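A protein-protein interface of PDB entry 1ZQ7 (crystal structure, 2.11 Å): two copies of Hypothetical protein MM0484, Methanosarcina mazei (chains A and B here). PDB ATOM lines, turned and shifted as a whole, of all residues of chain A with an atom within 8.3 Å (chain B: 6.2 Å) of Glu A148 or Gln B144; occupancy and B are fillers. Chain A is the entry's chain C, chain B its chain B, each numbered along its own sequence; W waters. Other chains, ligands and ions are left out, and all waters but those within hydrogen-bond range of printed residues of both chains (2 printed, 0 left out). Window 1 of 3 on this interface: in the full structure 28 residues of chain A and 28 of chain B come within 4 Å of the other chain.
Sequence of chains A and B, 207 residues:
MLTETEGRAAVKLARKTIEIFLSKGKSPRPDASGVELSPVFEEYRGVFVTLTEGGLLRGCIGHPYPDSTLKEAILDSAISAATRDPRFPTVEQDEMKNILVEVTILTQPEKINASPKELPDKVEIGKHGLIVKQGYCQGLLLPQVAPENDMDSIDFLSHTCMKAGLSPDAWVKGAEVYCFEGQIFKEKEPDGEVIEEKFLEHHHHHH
Leu A142 touches Glu B148, and with the chains exchanged Glu A148 touches Leu B142.
Leu A142 touches His B203, and with the chains exchanged His A203 touches Leu B142.
Gln A144 touches Glu B148, and with the chains exchanged Glu A148 touches Gln B144.
His B202 touches its own counterpart, His A202.
The backbone NH of Leu B142 sits at hydrogen-bond distance from the side-chain amide oxygen of Asn A149 (2.9 Å).
NE2 of Gln B144 lies within hydrogen-bond range of OE1 of Glu A148, 3.3 Å away.
OE1 of Glu B148 lies within hydrogen-bond range of NE2 of Gln A144 (3.4 Å).
The backbone NH (N) of Leu A142 is in hydrogen-bond range of the side-chain amide oxygen (OD1) of Asn B149 (3.1 Å).
Of the printed residues of chain B, Leu A142 touches Glu B148, Asn B149 and His B203.
Of chain B, only Leu B142 and Gln B144 come within 4 Å of Glu A148.
His A204 touches none of the printed residues of chain B.
Of the printed residues of chain A, Phe B48 touches His A203 (3.3 Å).
Printed residues of chain A within 4 Å of Leu B141: Asn A149 (3.4 Å).
No residue of chain A comes within 4 Å of Pro B143.
Of the printed residues of chain A, Gln B144 touches Glu A148 (3.3 Å).
Of the printed residues of chain A, Asn B149 touches Leu A142 and Val A145.
The nearest residue of chain B that does not touch Glu A148 is Glu B148 (5.3 Å).
The nearest printed residue of chain A that does not touch Leu B141 is Met A151 (4.1 Å).
Water W1 lies within hydrogen-bond range of a ring nitrogen (NE2) of His B203 (2.8 Å) and the side-chain amide nitrogen (NE2) of Gln A144 (3.2 Å).
Water W2 bridges NE2 of Gln B144 (3.1 Å) and NE2 of His A203 (3.2 Å).
Hydrophobic or aromatic side chains of chain B that line the printed part of chain A: Phe B48, Leu B141, Leu B142, Val B145, His B202 and His B203.
Hydrophobic or aromatic side chains of chain A within 4 Å of the printed part of chain B: Leu A142, Val A145, His A202 and His A203.
Among the printed residues, 13 pairs touch across the chains.
Among the printed residues, no Asp or Glu carboxylate lies within 4 Å of a Lys or Arg side-chain nitrogen of the other chain.
The backbone carbonyl oxygen of Val B145 sits at hydrogen-bond distance from the side-chain amide nitrogen of Asn B149.
The side-chain carboxylate of Glu B148 lies within hydrogen-bond range of the backbone NH of His B202 (2.8 Å).
N of Glu B148 sits at hydrogen-bond distance from O of His B203, 3.5 Å away.
The backbone carbonyl oxygen (O) of Val A145 sits at hydrogen-bond distance from the side-chain amide nitrogen (ND2) of Asn A149 (2.9 Å).
The side-chain carboxylate of Glu A148 lies within hydrogen-bond range of the backbone NH of His A202.
Leu A142 touches Glu B148.
CD1 of Leu A142 touches CE1 of His B203, at 3.6 Å.
Val A145 touches Asn B149.
Leu B142 touches Glu A148.
Leu B141 touches Asn A149.
Asn A149 touches Val B145 (ND2 to CG2, 3.2 Å).
NE2 of His A202 touches NE2 of His B202, 3.8 Å away.
His A203 touches Phe B48.
Leu B142 touches His A203 (CD1 to NE2, 3.6 Å).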
ATOM      1  N   ILE A 125       0.788 -14.261 -17.998  1.00  0.00           N
ATOM      2  CA  ILE A 125       0.304 -15.600 -17.700  1.00  0.00           C
ATOM      3  C   ILE A 125       0.279 -15.819 -16.192  1.00  0.00           C
ATOM      4  O   ILE A 125       1.293 -15.641 -15.517  1.00  0.00           O
ATOM      5  CB  ILE A 125       1.205 -16.662 -18.366  1.00  0.00           C
ATOM      6  CG1 ILE A 125       1.233 -16.426 -19.878  1.00  0.00           C
ATOM      7  CG2 ILE A 125       0.698 -18.066 -18.049  1.00  0.00           C
ATOM      8  CD1 ILE A 125      -0.138 -16.460 -20.524  1.00  0.00           C
ATOM      9  N   GLY A 126      -0.883 -16.201 -15.671  1.00  0.00           N
ATOM     10  CA  GLY A 126      -1.019 -16.436 -14.243  1.00  0.00           C
ATOM     11  C   GLY A 126      -1.911 -15.392 -13.601  1.00  0.00           C
ATOM     12  O   GLY A 126      -2.608 -15.656 -12.621  1.00  0.00           O
ATOM     13  N   LEU A 142     -10.488 -18.270 -18.871  1.00  0.00           N
ATOM     14  CA  LEU A 142     -10.178 -17.931 -17.488  1.00  0.00           C
ATOM     15  C   LEU A 142      -8.674 -17.812 -17.231  1.00  0.00           C
ATOM     16  O   LEU A 142      -7.858 -18.432 -17.922  1.00  0.00           O
ATOM     17  CB  LEU A 142     -10.831 -18.964 -16.559  1.00  0.00           C
ATOM     18  CG  LEU A 142     -12.369 -18.935 -16.633  1.00  0.00           C
ATOM     19  CD1 LEU A 142     -12.964 -20.173 -15.976  1.00  0.00           C
ATOM     20  CD2 LEU A 142     -12.883 -17.661 -15.964  1.00  0.00           C
ATOM     21  N   PRO A 143      -8.286 -17.000 -16.234  1.00  0.00           N
ATOM     22  CA  PRO A 143      -6.876 -16.791 -15.892  1.00  0.00           C
ATOM     23  C   PRO A 143      -6.079 -18.065 -15.690  1.00  0.00           C
ATOM     24  O   PRO A 143      -4.933 -18.168 -16.134  1.00  0.00           O
ATOM     25  CB  PRO A 143      -6.944 -15.962 -14.603  1.00  0.00           C
ATOM     26  CG  PRO A 143      -8.236 -15.218 -14.741  1.00  0.00           C
ATOM     27  CD  PRO A 143      -9.164 -16.283 -15.297  1.00  0.00           C
ATOM     28  N   GLN A 144      -6.691 -19.033 -15.020  1.00  0.00           N
ATOM     29  CA  GLN A 144      -6.028 -20.293 -14.709  1.00  0.00           C
ATOM     30  C   GLN A 144      -5.730 -21.186 -15.906  1.00  0.00           C
ATOM     31  O   GLN A 144      -4.940 -22.129 -15.795  1.00  0.00           O
ATOM     32  CB  GLN A 144      -6.859 -21.089 -13.690  1.00  0.00           C
ATOM     33  CG  GLN A 144      -8.189 -21.608 -14.234  1.00  0.00           C
ATOM     34  CD  GLN A 144      -9.373 -20.704 -13.897  1.00  0.00           C
ATOM     35  OE1 GLN A 144      -9.224 -19.494 -13.705  1.00  0.00           O
ATOM     36  NE2 GLN A 144     -10.560 -21.295 -13.845  1.00  0.00           N
ATOM     37  N   VAL A 145      -6.335 -20.900 -17.054  1.00  0.00           N
ATOM     38  CA  VAL A 145      -6.099 -21.758 -18.207  1.00  0.00           C
ATOM     39  C   VAL A 145      -4.651 -21.815 -18.685  1.00  0.00           C
ATOM     40  O   VAL A 145      -4.089 -22.901 -18.831  1.00  0.00           O
ATOM     41  CB  VAL A 145      -6.985 -21.377 -19.394  1.00  0.00           C
ATOM     42  CG1 VAL A 145      -6.704 -22.321 -20.551  1.00  0.00           C
ATOM     43  CG2 VAL A 145      -8.457 -21.456 -18.998  1.00  0.00           C
ATOM     44  N   ALA A 146      -4.046 -20.660 -18.929  1.00  0.00           N
ATOM     45  CA  ALA A 146      -2.668 -20.621 -19.417  1.00  0.00           C
ATOM     46  C   ALA A 146      -1.637 -21.282 -18.490  1.00  0.00           C
ATOM     47  O   ALA A 146      -0.916 -22.190 -18.903  1.00  0.00           O
ATOM     48  CB  ALA A 146      -2.265 -19.178 -19.715  1.00  0.00           C
ATOM     49  N   PRO A 147      -1.545 -20.827 -17.228  1.00  0.00           N
ATOM     50  CA  PRO A 147      -0.586 -21.411 -16.285  1.00  0.00           C
ATOM     51  C   PRO A 147      -0.720 -22.913 -16.084  1.00  0.00           C
ATOM     52  O   PRO A 147       0.278 -23.624 -16.058  1.00  0.00           O
ATOM     53  CB  PRO A 147      -0.840 -20.633 -14.994  1.00  0.00           C
ATOM     54  CG  PRO A 147      -2.258 -20.115 -15.162  1.00  0.00           C
ATOM     55  CD  PRO A 147      -2.283 -19.714 -16.602  1.00  0.00           C
ATOM     56  N   GLU A 148      -1.954 -23.390 -15.951  1.00  0.00           N
ATOM     57  CA  GLU A 148      -2.212 -24.804 -15.734  1.00  0.00           C
ATOM     58  C   GLU A 148      -2.001 -25.689 -16.959  1.00  0.00           C
ATOM     59  O   GLU A 148      -1.914 -26.903 -16.823  1.00  0.00           O
ATOM     60  CB  GLU A 148      -3.636 -25.001 -15.200  1.00  0.00           C
ATOM     61  CG  GLU A 148      -3.852 -24.413 -13.808  1.00  0.00           C
ATOM     62  CD  GLU A 148      -5.268 -24.573 -13.299  1.00  0.00           C
ATOM     63  OE1 GLU A 148      -6.113 -25.141 -14.024  1.00  0.00           O
ATOM     64  OE2 GLU A 148      -5.536 -24.126 -12.166  1.00  0.00           O
ATOM     65  N   ASN A 149      -1.915 -25.103 -18.152  1.00  0.00           N
ATOM     66  CA  ASN A 149      -1.723 -25.917 -19.352  1.00  0.00           C
ATOM     67  C   ASN A 149      -0.524 -25.516 -20.201  1.00  0.00           C
ATOM     68  O   ASN A 149      -0.520 -25.687 -21.416  1.00  0.00           O
ATOM     69  CB  ASN A 149      -3.002 -25.911 -20.186  1.00  0.00           C
ATOM     70  CG  ASN A 149      -4.171 -26.539 -19.446  1.00  0.00           C
ATOM     71  OD1 ASN A 149      -4.325 -27.765 -19.426  1.00  0.00           O
ATOM     72  ND2 ASN A 149      -4.986 -25.702 -18.810  1.00  0.00           N
ATOM     73  N   ASP A 150       0.492 -24.978 -19.535  1.00  0.00           N
ATOM     74  CA  ASP A 150       1.742 -24.584 -20.170  1.00  0.00           C
ATOM     75  C   ASP A 150       1.610 -23.733 -21.431  1.00  0.00           C
ATOM     76  O   ASP A 150       2.249 -24.023 -22.444  1.00  0.00           O
ATOM     77  CB  ASP A 150       2.559 -25.845 -20.480  1.00  0.00           C
ATOM     78  CG  ASP A 150       4.047 -25.568 -20.589  1.00  0.00           C
ATOM     79  OD1 ASP A 150       4.589 -24.857 -19.715  1.00  0.00           O
ATOM     80  OD2 ASP A 150       4.683 -26.074 -21.538  1.00  0.00           O
ATOM     81  N   MET A 151       0.794 -22.686 -21.377  1.00  0.00           N
ATOM     82  CA  MET A 151       0.639 -21.802 -22.531  1.00  0.00           C
ATOM     83  C   MET A 151       1.385 -20.500 -22.259  1.00  0.00           C
ATOM     84  O   MET A 151       1.363 -20.014 -21.130  1.00  0.00           O
ATOM     85  CB  MET A 151      -0.828 -21.441 -22.759  1.00  0.00           C
ATOM     86  CG  MET A 151      -1.794 -22.571 -22.976  1.00  0.00           C
ATOM     87  SD  MET A 151      -3.522 -21.754 -23.329  1.00  0.00           S
ATOM     88  CE  MET A 151      -4.467 -23.347 -23.903  1.00  0.00           C
ATOM     89  N   PHE A 199      -4.693 -16.637  -5.602  1.00  0.00           N
ATOM     90  CA  PHE A 199      -4.347 -17.507  -6.728  1.00  0.00           C
ATOM     91  C   PHE A 199      -5.535 -18.260  -7.326  1.00  0.00           C
ATOM     92  O   PHE A 199      -6.139 -19.102  -6.666  1.00  0.00           O
ATOM     93  CB  PHE A 199      -3.277 -18.508  -6.290  1.00  0.00           C
ATOM     94  CG  PHE A 199      -1.960 -17.879  -5.966  1.00  0.00           C
ATOM     95  CD1 PHE A 199      -1.107 -17.465  -6.985  1.00  0.00           C
ATOM     96  CD2 PHE A 199      -1.582 -17.664  -4.644  1.00  0.00           C
ATOM     97  CE1 PHE A 199       0.112 -16.846  -6.693  1.00  0.00           C
ATOM     98  CE2 PHE A 199      -0.366 -17.046  -4.338  1.00  0.00           C
ATOM     99  CZ  PHE A 199       0.483 -16.635  -5.365  1.00  0.00           C
ATOM    100  N   LEU A 200      -5.863 -17.953  -8.577  1.00  0.00           N
ATOM    101  CA  LEU A 200      -6.963 -18.620  -9.265  1.00  0.00           C
ATOM    102  C   LEU A 200      -6.490 -19.925  -9.901  1.00  0.00           C
ATOM    103  O   LEU A 200      -7.303 -20.784 -10.234  1.00  0.00           O
ATOM    104  CB  LEU A 200      -7.573 -17.708 -10.344  1.00  0.00           C
ATOM    105  CG  LEU A 200      -8.721 -16.773  -9.925  1.00  0.00           C
ATOM    106  CD1 LEU A 200      -8.225 -15.813  -8.862  1.00  0.00           C
ATOM    107  CD2 LEU A 200      -9.261 -16.002 -11.137  1.00  0.00           C
ATOM    108  N   GLU A 201      -5.177 -20.068 -10.070  1.00  0.00           N
ATOM    109  CA  GLU A 201      -4.618 -21.281 -10.666  1.00  0.00           C
ATOM    110  C   GLU A 201      -3.997 -22.192  -9.612  1.00  0.00           C
ATOM    111  O   GLU A 201      -3.338 -21.723  -8.684  1.00  0.00           O
ATOM    112  CB  GLU A 201      -3.561 -20.933 -11.728  1.00  0.00           C
ATOM    113  CG  GLU A 201      -2.166 -20.608 -11.199  1.00  0.00           C
ATOM    114  CD  GLU A 201      -2.101 -19.312 -10.412  1.00  0.00           C
ATOM    115  OE1 GLU A 201      -3.109 -18.578 -10.371  1.00  0.00           O
ATOM    116  OE2 GLU A 201      -1.028 -19.027  -9.839  1.00  0.00           O
ATOM    117  N   HIS A 202      -4.216 -23.497  -9.764  1.00  0.00           N
ATOM    118  CA  HIS A 202      -3.670 -24.484  -8.837  1.00  0.00           C
ATOM    119  C   HIS A 202      -2.161 -24.561  -9.002  1.00  0.00           C
ATOM    120  O   HIS A 202      -1.420 -24.575  -8.023  1.00  0.00           O
ATOM    121  CB  HIS A 202      -4.265 -25.875  -9.102  1.00  0.00           C
ATOM    122  CG  HIS A 202      -5.738 -25.976  -8.830  1.00  0.00           C
ATOM    123  ND1 HIS A 202      -6.632 -26.433  -9.767  1.00  0.00           N
ATOM    124  CD2 HIS A 202      -6.455 -25.706  -7.711  1.00  0.00           C
ATOM    125  CE1 HIS A 202      -7.850 -26.444  -9.240  1.00  0.00           C
ATOM    126  NE2 HIS A 202      -7.767 -26.010  -7.999  1.00  0.00           N
ATOM    127  N   HIS A 203      -1.716 -24.612 -10.253  1.00  0.00           N
ATOM    128  CA  HIS A 203      -0.298 -24.709 -10.560  1.00  0.00           C
ATOM    129  C   HIS A 203       0.095 -23.828 -11.744  1.00  0.00           C
ATOM    130  O   HIS A 203      -0.756 -23.375 -12.507  1.00  0.00           O
ATOM    131  CB  HIS A 203       0.066 -26.173 -10.818  1.00  0.00           C
ATOM    132  CG  HIS A 203      -0.864 -26.875 -11.758  1.00  0.00           C
ATOM    133  ND1 HIS A 203      -0.664 -26.904 -13.121  1.00  0.00           N
ATOM    134  CD2 HIS A 203      -2.008 -27.565 -11.531  1.00  0.00           C
ATOM    135  CE1 HIS A 203      -1.642 -27.585 -13.694  1.00  0.00           C
ATOM    136  NE2 HIS A 203      -2.470 -27.997 -12.750  1.00  0.00           N
ATOM    137  N   HIS A 204       1.395 -23.596 -11.887  1.00  0.00           N
ATOM    138  CA  HIS A 204       1.927 -22.740 -12.941  1.00  0.00           C
ATOM    139  C   HIS A 204       3.341 -23.215 -13.297  1.00  0.00           C
ATOM    140  O   HIS A 204       4.307 -22.615 -12.785  1.00  0.00           O
ATOM    141  CB  HIS A 204       1.952 -21.294 -12.422  1.00  0.00           C
ATOM    142  CG  HIS A 204       2.271 -20.268 -13.464  1.00  0.00           C
ATOM    143  ND1 HIS A 204       2.411 -20.575 -14.799  1.00  0.00           N
ATOM    144  CD2 HIS A 204       2.467 -18.930 -13.363  1.00  0.00           C
ATOM    145  CE1 HIS A 204       2.680 -19.472 -15.478  1.00  0.00           C
ATOM    146  NE2 HIS A 204       2.720 -18.462 -14.627  1.00  0.00           N
ATOM    147  N   PHE B  48      -0.380 -34.506  -9.406  1.00  0.00           N
ATOM    148  CA  PHE B  48      -0.117 -33.182  -8.867  1.00  0.00           C
ATOM    149  C   PHE B  48      -0.250 -33.269  -7.354  1.00  0.00           C
ATOM    150  O   PHE B  48      -1.130 -33.956  -6.846  1.00  0.00           O
ATOM    151  CB  PHE B  48      -1.117 -32.150  -9.404  1.00  0.00           C
ATOM    152  CG  PHE B  48      -0.909 -31.789 -10.847  1.00  0.00           C
ATOM    153  CD1 PHE B  48      -1.311 -32.651 -11.863  1.00  0.00           C
ATOM    154  CD2 PHE B  48      -0.283 -30.594 -11.192  1.00  0.00           C
ATOM    155  CE1 PHE B  48      -1.101 -32.325 -13.206  1.00  0.00           C
ATOM    156  CE2 PHE B  48      -0.065 -30.256 -12.530  1.00  0.00           C
ATOM    157  CZ  PHE B  48      -0.473 -31.128 -13.542  1.00  0.00           C
ATOM    158  N   PRO B  64       2.106 -33.429 -15.618  1.00  0.00           N
ATOM    159  CA  PRO B  64       0.893 -33.575 -16.433  1.00  0.00           C
ATOM    160  C   PRO B  64       0.928 -34.855 -17.273  1.00  0.00           C
ATOM    161  O   PRO B  64      -0.090 -35.531 -17.438  1.00  0.00           O
ATOM    162  CB  PRO B  64       0.911 -32.329 -17.317  1.00  0.00           C
ATOM    163  CG  PRO B  64       1.674 -31.334 -16.503  1.00  0.00           C
ATOM    164  CD  PRO B  64       2.792 -32.164 -15.918  1.00  0.00           C
ATOM    165  N   HIS B 128     -13.085 -36.304 -19.336  1.00  0.00           N
ATOM    166  CA  HIS B 128     -11.846 -36.471 -20.079  1.00  0.00           C
ATOM    167  C   HIS B 128     -10.853 -35.322 -20.203  1.00  0.00           C
ATOM    168  O   HIS B 128     -11.214 -34.151 -20.262  1.00  0.00           O
ATOM    169  CB  HIS B 128     -12.174 -36.968 -21.486  1.00  0.00           C
ATOM    170  CG  HIS B 128     -12.665 -38.382 -21.532  1.00  0.00           C
ATOM    171  ND1 HIS B 128     -13.615 -38.807 -22.429  1.00  0.00           N
ATOM    172  CD2 HIS B 128     -12.300 -39.472 -20.813  1.00  0.00           C
ATOM    173  CE1 HIS B 128     -13.821 -40.107 -22.263  1.00  0.00           C
ATOM    174  NE2 HIS B 128     -13.036 -40.530 -21.292  1.00  0.00           N
ATOM    175  N   LEU B 141      -4.288 -30.958 -22.574  1.00  0.00           N
ATOM    176  CA  LEU B 141      -5.118 -30.036 -21.821  1.00  0.00           C
ATOM    177  C   LEU B 141      -5.782 -30.856 -20.723  1.00  0.00           C
ATOM    178  O   LEU B 141      -6.329 -31.930 -20.980  1.00  0.00           O
ATOM    179  CB  LEU B 141      -6.154 -29.396 -22.751  1.00  0.00           C
ATOM    180  CG  LEU B 141      -5.458 -28.607 -23.869  1.00  0.00           C
ATOM    181  CD1 LEU B 141      -6.465 -28.148 -24.913  1.00  0.00           C
ATOM    182  CD2 LEU B 141      -4.725 -27.406 -23.251  1.00  0.00           C
ATOM    183  N   LEU B 142      -5.705 -30.370 -19.491  1.00  0.00           N
ATOM    184  CA  LEU B 142      -6.289 -31.094 -18.370  1.00  0.00           C
ATOM    185  C   LEU B 142      -7.798 -31.161 -18.508  1.00  0.00           C
ATOM    186  O   LEU B 142      -8.397 -30.349 -19.215  1.00  0.00           O
ATOM    187  CB  LEU B 142      -5.897 -30.421 -17.055  1.00  0.00           C
ATOM    188  CG  LEU B 142      -4.380 -30.407 -16.841  1.00  0.00           C
ATOM    189  CD1 LEU B 142      -4.014 -29.492 -15.672  1.00  0.00           C
ATOM    190  CD2 LEU B 142      -3.898 -31.818 -16.593  1.00  0.00           C
ATOM    191  N   PRO B 143      -8.436 -32.124 -17.825  1.00  0.00           N
ATOM    192  CA  PRO B 143      -9.891 -32.304 -17.871  1.00  0.00           C
ATOM    193  C   PRO B 143     -10.745 -31.075 -17.548  1.00  0.00           C
ATOM    194  O   PRO B 143     -11.793 -30.871 -18.169  1.00  0.00           O
ATOM    195  CB  PRO B 143     -10.135 -33.430 -16.864  1.00  0.00           C
ATOM    196  CG  PRO B 143      -8.850 -34.202 -16.886  1.00  0.00           C
ATOM    197  CD  PRO B 143      -7.815 -33.118 -16.931  1.00  0.00           C
ATOM    198  N   GLN B 144     -10.311 -30.261 -16.582  1.00  0.00           N
ATOM    199  CA  GLN B 144     -11.089 -29.088 -16.176  1.00  0.00           C
ATOM    200  C   GLN B 144     -11.190 -27.995 -17.231  1.00  0.00           C
ATOM    201  O   GLN B 144     -12.114 -27.181 -17.201  1.00  0.00           O
ATOM    202  CB  GLN B 144     -10.538 -28.477 -14.869  1.00  0.00           C
ATOM    203  CG  GLN B 144      -9.128 -27.899 -14.942  1.00  0.00           C
ATOM    204  CD  GLN B 144      -8.060 -28.892 -14.516  1.00  0.00           C
ATOM    205  OE1 GLN B 144      -8.251 -30.101 -14.610  1.00  0.00           O
ATOM    206  NE2 GLN B 144      -6.923 -28.381 -14.057  1.00  0.00           N
ATOM    207  N   VAL B 145     -10.255 -27.983 -18.174  1.00  0.00           N
ATOM    208  CA  VAL B 145     -10.259 -26.957 -19.207  1.00  0.00           C
ATOM    209  C   VAL B 145     -11.570 -26.837 -19.988  1.00  0.00           C
ATOM    210  O   VAL B 145     -12.157 -25.755 -20.060  1.00  0.00           O
ATOM    211  CB  VAL B 145      -9.100 -27.183 -20.203  1.00  0.00           C
ATOM    212  CG1 VAL B 145      -9.163 -26.152 -21.334  1.00  0.00           C
ATOM    213  CG2 VAL B 145      -7.771 -27.100 -19.468  1.00  0.00           C
ATOM    214  N   ALA B 146     -12.038 -27.940 -20.556  1.00  0.00           N
ATOM    215  CA  ALA B 146     -13.260 -27.920 -21.365  1.00  0.00           C
ATOM    216  C   ALA B 146     -14.535 -27.462 -20.647  1.00  0.00           C
ATOM    217  O   ALA B 146     -15.217 -26.554 -21.117  1.00  0.00           O
ATOM    218  CB  ALA B 146     -13.484 -29.299 -22.008  1.00  0.00           C
ATOM    219  N   PRO B 147     -14.872 -28.083 -19.500  1.00  0.00           N
ATOM    220  CA  PRO B 147     -16.084 -27.696 -18.767  1.00  0.00           C
ATOM    221  C   PRO B 147     -16.046 -26.300 -18.167  1.00  0.00           C
ATOM    222  O   PRO B 147     -17.057 -25.596 -18.179  1.00  0.00           O
ATOM    223  CB  PRO B 147     -16.204 -28.777 -17.704  1.00  0.00           C
ATOM    224  CG  PRO B 147     -14.758 -29.109 -17.413  1.00  0.00           C
ATOM    225  CD  PRO B 147     -14.159 -29.166 -18.803  1.00  0.00           C
ATOM    226  N   GLU B 148     -14.889 -25.899 -17.645  1.00  0.00           N
ATOM    227  CA  GLU B 148     -14.743 -24.574 -17.052  1.00  0.00           C
ATOM    228  C   GLU B 148     -14.699 -23.461 -18.088  1.00  0.00           C
ATOM    229  O   GLU B 148     -14.873 -22.295 -17.753  1.00  0.00           O
ATOM    230  CB  GLU B 148     -13.472 -24.509 -16.203  1.00  0.00           C
ATOM    231  CG  GLU B 148     -13.561 -25.280 -14.896  1.00  0.00           C
ATOM    232  CD  GLU B 148     -12.273 -25.227 -14.102  1.00  0.00           C
ATOM    233  OE1 GLU B 148     -11.330 -24.529 -14.534  1.00  0.00           O
ATOM    234  OE2 GLU B 148     -12.205 -25.885 -13.044  1.00  0.00           O
ATOM    235  N   ASN B 149     -14.463 -23.805 -19.351  1.00  0.00           N
ATOM    236  CA  ASN B 149     -14.393 -22.768 -20.368  1.00  0.00           C
ATOM    237  C   ASN B 149     -15.385 -22.957 -21.495  1.00  0.00           C
ATOM    238  O   ASN B 149     -15.180 -22.508 -22.622  1.00  0.00           O
ATOM    239  CB  ASN B 149     -12.961 -22.655 -20.878  1.00  0.00           C
ATOM    240  CG  ASN B 149     -12.018 -22.137 -19.804  1.00  0.00           C
ATOM    241  OD1 ASN B 149     -11.985 -20.935 -19.509  1.00  0.00           O
ATOM    242  ND2 ASN B 149     -11.265 -23.045 -19.198  1.00  0.00           N
ATOM    243  N   PHE B 156     -12.756 -28.993 -27.785  1.00  0.00           N
ATOM    244  CA  PHE B 156     -11.669 -29.591 -27.014  1.00  0.00           C
ATOM    245  C   PHE B 156     -10.629 -30.279 -27.884  1.00  0.00           C
ATOM    246  O   PHE B 156      -9.425 -30.126 -27.676  1.00  0.00           O
ATOM    247  CB  PHE B 156     -12.254 -30.565 -25.992  1.00  0.00           C
ATOM    248  CG  PHE B 156     -11.391 -30.770 -24.775  1.00  0.00           C
ATOM    249  CD1 PHE B 156     -10.478 -29.797 -24.370  1.00  0.00           C
ATOM    250  CD2 PHE B 156     -11.531 -31.916 -24.004  1.00  0.00           C
ATOM    251  CE1 PHE B 156      -9.723 -29.963 -23.214  1.00  0.00           C
ATOM    252  CE2 PHE B 156     -10.779 -32.095 -22.840  1.00  0.00           C
ATOM    253  CZ  PHE B 156      -9.874 -31.117 -22.445  1.00  0.00           C
ATOM    254  N   LEU B 200     -12.823 -32.744 -11.018  1.00  0.00           N
ATOM    255  CA  LEU B 200     -11.597 -31.965 -11.155  1.00  0.00           C
ATOM    256  C   LEU B 200     -11.917 -30.528 -11.546  1.00  0.00           C
ATOM    257  O   LEU B 200     -11.106 -29.633 -11.335  1.00  0.00           O
ATOM    258  CB  LEU B 200     -10.666 -32.573 -12.205  1.00  0.00           C
ATOM    259  CG  LEU B 200      -9.488 -33.426 -11.722  1.00  0.00           C
ATOM    260  CD1 LEU B 200      -9.980 -34.575 -10.856  1.00  0.00           C
ATOM    261  CD2 LEU B 200      -8.723 -33.960 -12.928  1.00  0.00           C
ATOM    262  N   GLU B 201     -13.099 -30.302 -12.117  1.00  0.00           N
ATOM    263  CA  GLU B 201     -13.458 -28.954 -12.519  1.00  0.00           C
ATOM    264  C   GLU B 201     -14.351 -28.260 -11.495  1.00  0.00           C
ATOM    265  O   GLU B 201     -15.166 -28.894 -10.829  1.00  0.00           O
ATOM    266  CB  GLU B 201     -14.144 -28.958 -13.896  1.00  0.00           C
ATOM    267  CG  GLU B 201     -15.638 -29.278 -13.905  1.00  0.00           C
ATOM    268  CD  GLU B 201     -15.938 -30.720 -13.573  1.00  0.00           C
ATOM    269  OE1 GLU B 201     -15.021 -31.558 -13.704  1.00  0.00           O
ATOM    270  OE2 GLU B 201     -17.092 -31.017 -13.194  1.00  0.00           O
ATOM    271  N   HIS B 202     -14.182 -26.949 -11.372  1.00  0.00           N
ATOM    272  CA  HIS B 202     -14.970 -26.157 -10.437  1.00  0.00           C
ATOM    273  C   HIS B 202     -16.412 -26.042 -10.927  1.00  0.00           C
ATOM    274  O   HIS B 202     -17.366 -26.274 -10.177  1.00  0.00           O
ATOM    275  CB  HIS B 202     -14.360 -24.758 -10.302  1.00  0.00           C
ATOM    276  CG  HIS B 202     -13.069 -24.729  -9.548  1.00  0.00           C
ATOM    277  ND1 HIS B 202     -12.085 -23.780  -9.788  1.00  0.00           N
ATOM    278  CD2 HIS B 202     -12.604 -25.483  -8.526  1.00  0.00           C
ATOM    279  CE1 HIS B 202     -11.087 -23.959  -8.951  1.00  0.00           C
ATOM    280  NE2 HIS B 202     -11.375 -24.991  -8.167  1.00  0.00           N
ATOM    281  N   HIS B 203     -16.563 -25.693 -12.198  1.00  0.00           N
ATOM    282  CA  HIS B 203     -17.879 -25.524 -12.795  1.00  0.00           C
ATOM    283  C   HIS B 203     -17.946 -26.157 -14.183  1.00  0.00           C
ATOM    284  O   HIS B 203     -16.924 -26.353 -14.836  1.00  0.00           O
ATOM    285  CB  HIS B 203     -18.215 -24.032 -12.858  1.00  0.00           C
ATOM    286  CG  HIS B 203     -17.054 -23.169 -13.252  1.00  0.00           C
ATOM    287  ND1 HIS B 203     -16.739 -22.896 -14.565  1.00  0.00           N
ATOM    288  CD2 HIS B 203     -16.115 -22.545 -12.501  1.00  0.00           C
ATOM    289  CE1 HIS B 203     -15.653 -22.142 -14.608  1.00  0.00           C
ATOM    290  NE2 HIS B 203     -15.254 -21.915 -13.370  1.00  0.00           N
HETATM  291  O   HOH W   1     -13.223 -20.395 -12.239  1.00  0.00           O
HETATM  292  O   HOH W   2      -4.924 -30.026 -12.289  1.00  0.00           O
